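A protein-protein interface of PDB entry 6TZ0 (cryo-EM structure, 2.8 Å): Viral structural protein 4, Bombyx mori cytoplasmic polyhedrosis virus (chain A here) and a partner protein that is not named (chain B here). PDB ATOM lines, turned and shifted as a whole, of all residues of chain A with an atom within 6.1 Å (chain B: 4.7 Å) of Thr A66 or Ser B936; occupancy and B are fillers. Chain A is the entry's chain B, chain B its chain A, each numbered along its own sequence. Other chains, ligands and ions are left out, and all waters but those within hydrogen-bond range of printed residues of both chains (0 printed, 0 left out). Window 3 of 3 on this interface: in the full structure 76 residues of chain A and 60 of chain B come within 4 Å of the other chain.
The backbone carbonyl oxygen (O) of Ala B454 is in hydrogen-bond range of the side-chain amide nitrogen (ND2) of Asn A64 (3.3 Å).
NH2 of Arg B458 is in hydrogen-bond range of OD1 of Asn A64.
The side-chain carboxylate (OE2) of Glu B932 sits at hydrogen-bond distance from the backbone NH (N) of Asn A64 (2.9 Å).
The side-chain amide nitrogen (ND2) of Asn A64 sits at hydrogen-bond distance from the side-chain hydroxyl (OG) of Ser B936, 3.1 Å away.
The backbone carbonyl oxygen of Ile A68 sits close to the side-chain amide nitrogen of Gln B939, 2.4 Å away.
The side-chain hydroxyl of Ser B936 sits at hydrogen-bond distance from the backbone carbonyl oxygen of Ala B454 (3.4 Å).
O of Leu B933 sits at hydrogen-bond distance from OG of Ser B936, at 2.8 Å.
The backbone carbonyl oxygen (O) of Thr B935 lies close to the side-chain amide oxygen (OE1) of Gln B939.
A ring nitrogen (ND1) of His A59 sits at hydrogen-bond distance from the guanidinium group (NH2) of Arg A62 (3.1 Å).
The backbone carbonyl oxygen (O) of Ala A60 sits close to the backbone NH (N) of Gly A65, at 3.3 Å.
The backbone NH (N) of Leu A67 lies within hydrogen-bond range of the side-chain amide oxygen (OE1) of Gln A174, 3.0 Å away.
Among the printed residues, merely in contact across the chains: Gly A65 with Arg B458 (3.3 Å), Asn A64 with Leu B933 (3.4 Å), Gln A174 with Arg B458 (3.6 Å), Leu A67 with Gln B939 (3.6 Å), Thr A66 with Ser B936 (3.6 Å), His A63 with Glu B932 (3.7 Å), Thr A66 with Arg B458 (3.7 Å) and Arg A62 with Glu B932 (3.8 Å).
Ala A60 touches none of the printed residues of chain B.
Ala A61 touches none of the printed residues of chain B.
Of the printed residues of chain B, Asn A64 touches Ala B454 (3.3 Å), Arg B458 (2.9 Å), Glu B932 (2.9 Å), Leu B933 (3.4 Å) and Ser B936 (3.1 Å).
Of the printed residues of chain B, Gly A65 touches Arg B458.
Of the printed residues of chain B, Gln A174 touches Arg B458 (3.6 Å).
Of the printed residues of chain A, Glu B932 touches Arg A62, His A63 and Asn A64.
Of the printed residues of chain A, Leu B933 touches Asn A64.
Ser B936 touches just these residues of chain A: Asn A64 and Thr A66.
The nearest residue of chain B that does not touch Thr A66 is Ala B457 (4.04 Å).
The nearest printed residue of chain A that does not touch Glu B932 is Gly A65 (5.5 Å).
Of the 11 printed residues of chain A, 8 touch a printed residue of chain B.
Along chain B the printed residues that touch a printed residue of chain A span positions 454 to 939.
Among the printed residues, 13 pairs touch across the chains.
Among the printed residues, no Asp or Glu carboxylate lies within 4 Å of a Lys or Arg side-chain nitrogen of the other chain.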
ATOM      1  N   HIS A  59      14.133  21.319 -27.717  1.00  0.00           N
ATOM      2  CA  HIS A  59      15.156  21.862 -26.826  1.00  0.00           C
ATOM      3  C   HIS A  59      14.771  21.725 -25.360  1.00  0.00           C
ATOM      4  O   HIS A  59      15.653  21.606 -24.506  1.00  0.00           O
ATOM      5  CB  HIS A  59      15.449  23.331 -27.117  1.00  0.00           C
ATOM      6  CG  HIS A  59      16.026  23.580 -28.471  1.00  0.00           C
ATOM      7  ND1 HIS A  59      17.183  22.978 -28.905  1.00  0.00           N
ATOM      8  CD2 HIS A  59      15.671  24.453 -29.440  1.00  0.00           C
ATOM      9  CE1 HIS A  59      17.474  23.413 -30.117  1.00  0.00           C
ATOM     10  NE2 HIS A  59      16.574  24.313 -30.462  1.00  0.00           N
ATOM     11  N   ALA A  60      13.479  21.764 -25.039  1.00  0.00           N
ATOM     12  CA  ALA A  60      13.066  21.619 -23.650  1.00  0.00           C
ATOM     13  C   ALA A  60      13.154  20.185 -23.163  1.00  0.00           C
ATOM     14  O   ALA A  60      13.314  19.967 -21.959  1.00  0.00           O
ATOM     15  CB  ALA A  60      11.639  22.132 -23.458  1.00  0.00           C
ATOM     16  N   ALA A  61      13.067  19.203 -24.062  1.00  0.00           N
ATOM     17  CA  ALA A  61      13.159  17.814 -23.629  1.00  0.00           C
ATOM     18  C   ALA A  61      14.554  17.404 -23.171  1.00  0.00           C
ATOM     19  O   ALA A  61      14.697  16.317 -22.607  1.00  0.00           O
ATOM     20  CB  ALA A  61      12.702  16.885 -24.749  1.00  0.00           C
ATOM     21  N   ARG A  62      15.579  18.229 -23.382  1.00  0.00           N
ATOM     22  CA  ARG A  62      16.939  17.832 -23.054  1.00  0.00           C
ATOM     23  C   ARG A  62      17.432  18.330 -21.705  1.00  0.00           C
ATOM     24  O   ARG A  62      18.397  17.768 -21.181  1.00  0.00           O
ATOM     25  CB  ARG A  62      17.921  18.308 -24.129  1.00  0.00           C
ATOM     26  CG  ARG A  62      17.756  17.610 -25.459  1.00  0.00           C
ATOM     27  CD  ARG A  62      19.016  17.722 -26.293  1.00  0.00           C
ATOM     28  NE  ARG A  62      19.337  19.087 -26.689  1.00  0.00           N
ATOM     29  CZ  ARG A  62      18.983  19.631 -27.848  1.00  0.00           C
ATOM     30  NH1 ARG A  62      18.304  18.925 -28.739  1.00  0.00           N
ATOM     31  NH2 ARG A  62      19.326  20.881 -28.123  1.00  0.00           N
ATOM     32  N   HIS A  63      16.827  19.369 -21.128  1.00  0.00           N
ATOM     33  CA  HIS A  63      17.279  19.890 -19.836  1.00  0.00           C
ATOM     34  C   HIS A  63      16.090  20.006 -18.895  1.00  0.00           C
ATOM     35  O   HIS A  63      15.579  21.110 -18.699  1.00  0.00           O
ATOM     36  CB  HIS A  63      17.958  21.235 -20.004  1.00  0.00           C
ATOM     37  CG  HIS A  63      19.208  21.189 -20.821  1.00  0.00           C
ATOM     38  ND1 HIS A  63      19.212  21.382 -22.186  1.00  0.00           N
ATOM     39  CD2 HIS A  63      20.496  20.974 -20.468  1.00  0.00           C
ATOM     40  CE1 HIS A  63      20.448  21.286 -22.638  1.00  0.00           C
ATOM     41  NE2 HIS A  63      21.246  21.033 -21.616  1.00  0.00           N
ATOM     42  N   ASN A  64      15.698  18.876 -18.298  1.00  0.00           N
ATOM     43  CA  ASN A  64      14.769  18.803 -17.164  1.00  0.00           C
ATOM     44  C   ASN A  64      13.411  19.457 -17.461  1.00  0.00           C
ATOM     45  O   ASN A  64      12.720  19.926 -16.558  1.00  0.00           O
ATOM     46  CB  ASN A  64      15.415  19.417 -15.914  1.00  0.00           C
ATOM     47  CG  ASN A  64      14.813  18.907 -14.623  1.00  0.00           C
ATOM     48  OD1 ASN A  64      13.947  18.038 -14.630  1.00  0.00           O
ATOM     49  ND2 ASN A  64      15.253  19.466 -13.507  1.00  0.00           N
ATOM     50  N   GLY A  65      13.012  19.507 -18.728  1.00  0.00           N
ATOM     51  CA  GLY A  65      11.779  20.179 -19.086  1.00  0.00           C
ATOM     52  C   GLY A  65      11.825  21.690 -19.060  1.00  0.00           C
ATOM     53  O   GLY A  65      10.767  22.324 -19.084  1.00  0.00           O
ATOM     54  N   THR A  66      13.011  22.293 -19.017  1.00  0.00           N
ATOM     55  CA  THR A  66      13.158  23.739 -18.936  1.00  0.00           C
ATOM     56  C   THR A  66      13.962  24.263 -20.117  1.00  0.00           C
ATOM     57  O   THR A  66      14.612  23.510 -20.842  1.00  0.00           O
ATOM     58  CB  THR A  66      13.846  24.169 -17.633  1.00  0.00           C
ATOM     59  OG1 THR A  66      15.156  23.594 -17.572  1.00  0.00           O
ATOM     60  CG2 THR A  66      13.051  23.739 -16.426  1.00  0.00           C
ATOM     61  N   LEU A  67      13.923  25.581 -20.289  1.00  0.00           N
ATOM     62  CA  LEU A  67      14.723  26.274 -21.285  1.00  0.00           C
ATOM     63  C   LEU A  67      15.842  27.045 -20.597  1.00  0.00           C
ATOM     64  O   LEU A  67      15.645  27.610 -19.519  1.00  0.00           O
ATOM     65  CB  LEU A  67      13.857  27.217 -22.120  1.00  0.00           C
ATOM     66  CG  LEU A  67      12.824  26.498 -22.982  1.00  0.00           C
ATOM     67  CD1 LEU A  67      11.877  27.487 -23.616  1.00  0.00           C
ATOM     68  CD2 LEU A  67      13.502  25.657 -24.038  1.00  0.00           C
ATOM     69  N   ILE A  68      17.014  27.070 -21.229  1.00  0.00           N
ATOM     70  CA  ILE A  68      18.232  27.480 -20.535  1.00  0.00           C
ATOM     71  C   ILE A  68      18.358  29.002 -20.456  1.00  0.00           C
ATOM     72  O   ILE A  68      19.021  29.531 -19.557  1.00  0.00           O
ATOM     73  CB  ILE A  68      19.436  26.803 -21.218  1.00  0.00           C
ATOM     74  CG1 ILE A  68      19.232  25.294 -21.202  1.00  0.00           C
ATOM     75  CG2 ILE A  68      20.755  27.066 -20.501  1.00  0.00           C
ATOM     76  CD1 ILE A  68      19.135  24.727 -19.802  1.00  0.00           C
ATOM     77  N   GLN A 174       7.067  29.058 -19.551  1.00  0.00           N
ATOM     78  CA  GLN A 174       8.364  29.651 -19.247  1.00  0.00           C
ATOM     79  C   GLN A 174       8.611  30.903 -20.077  1.00  0.00           C
ATOM     80  O   GLN A 174       9.281  31.830 -19.614  1.00  0.00           O
ATOM     81  CB  GLN A 174       9.464  28.621 -19.487  1.00  0.00           C
ATOM     82  CG  GLN A 174       9.350  27.419 -18.580  1.00  0.00           C
ATOM     83  CD  GLN A 174      10.274  26.295 -18.964  1.00  0.00           C
ATOM     84  OE1 GLN A 174      11.092  26.426 -19.866  1.00  0.00           O
ATOM     85  NE2 GLN A 174      10.097  25.155 -18.326  1.00  0.00           N
ATOM     86  N   ALA B 454      14.118  22.267  -7.360  1.00  0.00           N
ATOM     87  CA  ALA B 454      14.934  22.025  -8.543  1.00  0.00           C
ATOM     88  C   ALA B 454      14.394  20.880  -9.392  1.00  0.00           C
ATOM     89  O   ALA B 454      14.643  20.837 -10.600  1.00  0.00           O
ATOM     90  CB  ALA B 454      16.374  21.740  -8.131  1.00  0.00           C
ATOM     91  N   ALA B 457      11.010  22.214 -11.406  1.00  0.00           N
ATOM     92  CA  ALA B 457      11.200  23.574 -11.888  1.00  0.00           C
ATOM     93  C   ALA B 457      10.558  23.811 -13.244  1.00  0.00           C
ATOM     94  O   ALA B 457      10.360  24.966 -13.625  1.00  0.00           O
ATOM     95  CB  ALA B 457      12.687  23.895 -11.965  1.00  0.00           C
ATOM     96  N   ARG B 458      10.221  22.750 -13.977  1.00  0.00           N
ATOM     97  CA  ARG B 458       9.593  22.911 -15.280  1.00  0.00           C
ATOM     98  C   ARG B 458       8.150  23.371 -15.176  1.00  0.00           C
ATOM     99  O   ARG B 458       7.585  23.823 -16.175  1.00  0.00           O
ATOM    100  CB  ARG B 458       9.648  21.599 -16.059  1.00  0.00           C
ATOM    101  CG  ARG B 458       8.715  20.539 -15.533  1.00  0.00           C
ATOM    102  CD  ARG B 458       8.871  19.236 -16.281  1.00  0.00           C
ATOM    103  NE  ARG B 458      10.123  18.567 -15.944  1.00  0.00           N
ATOM    104  CZ  ARG B 458      10.550  17.445 -16.509  1.00  0.00           C
ATOM    105  NH1 ARG B 458       9.817  16.850 -17.436  1.00  0.00           N
ATOM    106  NH2 ARG B 458      11.704  16.912 -16.139  1.00  0.00           N
ATOM    107  N   GLU B 932      22.326  19.293 -13.946  1.00  0.00           N
ATOM    108  CA  GLU B 932      21.064  19.532 -14.634  1.00  0.00           C
ATOM    109  C   GLU B 932      20.025  20.151 -13.706  1.00  0.00           C
ATOM    110  O   GLU B 932      19.332  21.102 -14.095  1.00  0.00           O
ATOM    111  CB  GLU B 932      20.550  18.229 -15.237  1.00  0.00           C
ATOM    112  CG  GLU B 932      19.286  18.393 -16.045  1.00  0.00           C
ATOM    113  CD  GLU B 932      18.901  17.135 -16.779  1.00  0.00           C
ATOM    114  OE1 GLU B 932      19.640  16.135 -16.675  1.00  0.00           O
ATOM    115  OE2 GLU B 932      17.856  17.146 -17.462  1.00  0.00           O
ATOM    116  N   LEU B 933      19.934  19.657 -12.466  1.00  0.00           N
ATOM    117  CA  LEU B 933      18.981  20.216 -11.511  1.00  0.00           C
ATOM    118  C   LEU B 933      19.343  21.644 -11.125  1.00  0.00           C
ATOM    119  O   LEU B 933      18.461  22.506 -11.040  1.00  0.00           O
ATOM    120  CB  LEU B 933      18.894  19.342 -10.262  1.00  0.00           C
ATOM    121  CG  LEU B 933      18.248  17.963 -10.373  1.00  0.00           C
ATOM    122  CD1 LEU B 933      18.348  17.257  -9.044  1.00  0.00           C
ATOM    123  CD2 LEU B 933      16.809  18.058 -10.809  1.00  0.00           C
ATOM    124  N   ALA B 934      20.634  21.929 -10.933  1.00  0.00           N
ATOM    125  CA  ALA B 934      21.017  23.286 -10.551  1.00  0.00           C
ATOM    126  C   ALA B 934      20.881  24.264 -11.715  1.00  0.00           C
ATOM    127  O   ALA B 934      20.489  25.423 -11.515  1.00  0.00           O
ATOM    128  CB  ALA B 934      22.436  23.296 -10.007  1.00  0.00           C
ATOM    129  N   THR B 935      21.181  23.812 -12.937  1.00  0.00           N
ATOM    130  CA  THR B 935      21.000  24.643 -14.120  1.00  0.00           C
ATOM    131  C   THR B 935      19.528  24.962 -14.345  1.00  0.00           C
ATOM    132  O   THR B 935      19.180  26.088 -14.717  1.00  0.00           O
ATOM    133  CB  THR B 935      21.591  23.927 -15.336  1.00  0.00           C
ATOM    134  OG1 THR B 935      22.963  23.614 -15.081  1.00  0.00           O
ATOM    135  CG2 THR B 935      21.519  24.792 -16.576  1.00  0.00           C
ATOM    136  N   SER B 936      18.646  23.989 -14.102  1.00  0.00           N
ATOM    137  CA  SER B 936      17.219  24.256 -14.224  1.00  0.00           C
ATOM    138  C   SER B 936      16.712  25.145 -13.099  1.00  0.00           C
ATOM    139  O   SER B 936      15.776  25.923 -13.304  1.00  0.00           O
ATOM    140  CB  SER B 936      16.439  22.947 -14.249  1.00  0.00           C
ATOM    141  OG  SER B 936      16.533  22.285 -13.005  1.00  0.00           O
ATOM    142  N   LEU B 937      17.315  25.051 -11.913  1.00  0.00           N
ATOM    143  CA  LEU B 937      16.884  25.888 -10.800  1.00  0.00           C
ATOM    144  C   LEU B 937      17.302  27.340 -10.987  1.00  0.00           C
ATOM    145  O   LEU B 937      16.586  28.246 -10.549  1.00  0.00           O
ATOM    146  CB  LEU B 937      17.441  25.327  -9.495  1.00  0.00           C
ATOM    147  CG  LEU B 937      17.122  26.041  -8.188  1.00  0.00           C
ATOM    148  CD1 LEU B 937      15.630  26.139  -7.993  1.00  0.00           C
ATOM    149  CD2 LEU B 937      17.748  25.280  -7.054  1.00  0.00           C
ATOM    150  N   GLU B 938      18.431  27.584 -11.656  1.00  0.00           N
ATOM    151  CA  GLU B 938      18.877  28.953 -11.910  1.00  0.00           C
ATOM    152  C   GLU B 938      17.974  29.735 -12.853  1.00  0.00           C
ATOM    153  O   GLU B 938      18.122  30.957 -12.941  1.00  0.00           O
ATOM    154  CB  GLU B 938      20.280  28.964 -12.502  1.00  0.00           C
ATOM    155  CG  GLU B 938      21.360  28.562 -11.556  1.00  0.00           C
ATOM    156  CD  GLU B 938      22.722  28.610 -12.200  1.00  0.00           C
ATOM    157  OE1 GLU B 938      22.797  28.871 -13.419  1.00  0.00           O
ATOM    158  OE2 GLU B 938      23.724  28.379 -11.492  1.00  0.00           O
ATOM    159  N   GLN B 939      17.061  29.081 -13.564  1.00  0.00           N
ATOM    160  CA  GLN B 939      16.238  29.752 -14.552  1.00  0.00           C
ATOM    161  C   GLN B 939      14.931  30.274 -13.975  1.00  0.00           C
ATOM    162  O   GLN B 939      13.968  30.447 -14.726  1.00  0.00           O
ATOM    163  CB  GLN B 939      15.942  28.809 -15.716  1.00  0.00           C
ATOM    164  CG  GLN B 939      17.171  28.184 -16.325  1.00  0.00           C
ATOM    165  CD  GLN B 939      18.245  29.194 -16.612  1.00  0.00           C
ATOM    166  OE1 GLN B 939      19.322  29.152 -16.026  1.00  0.00           O
ATOM    167  NE2 GLN B 939      17.951  30.133 -17.496  1.00  0.00           N
ATOM    168  N   LEU B 940      14.865  30.519 -12.668  1.00  0.00           N
ATOM    169  CA  LEU B 940      13.595  30.844 -12.035  1.00  0.00           C
ATOM    170  C   LEU B 940      13.503  32.262 -11.503  1.00  0.00           C
ATOM    171  O   LEU B 940      12.402  32.706 -11.187  1.00  0.00           O
ATOM    172  CB  LEU B 940      13.297  29.871 -10.890  1.00  0.00           C
ATOM    173  CG  LEU B 940      13.095  28.405 -11.268  1.00  0.00           C
ATOM    174  CD1 LEU B 940      12.728  27.608 -10.038  1.00  0.00           C
ATOM    175  CD2 LEU B 940      12.058  28.244 -12.348  1.00  0.00           C
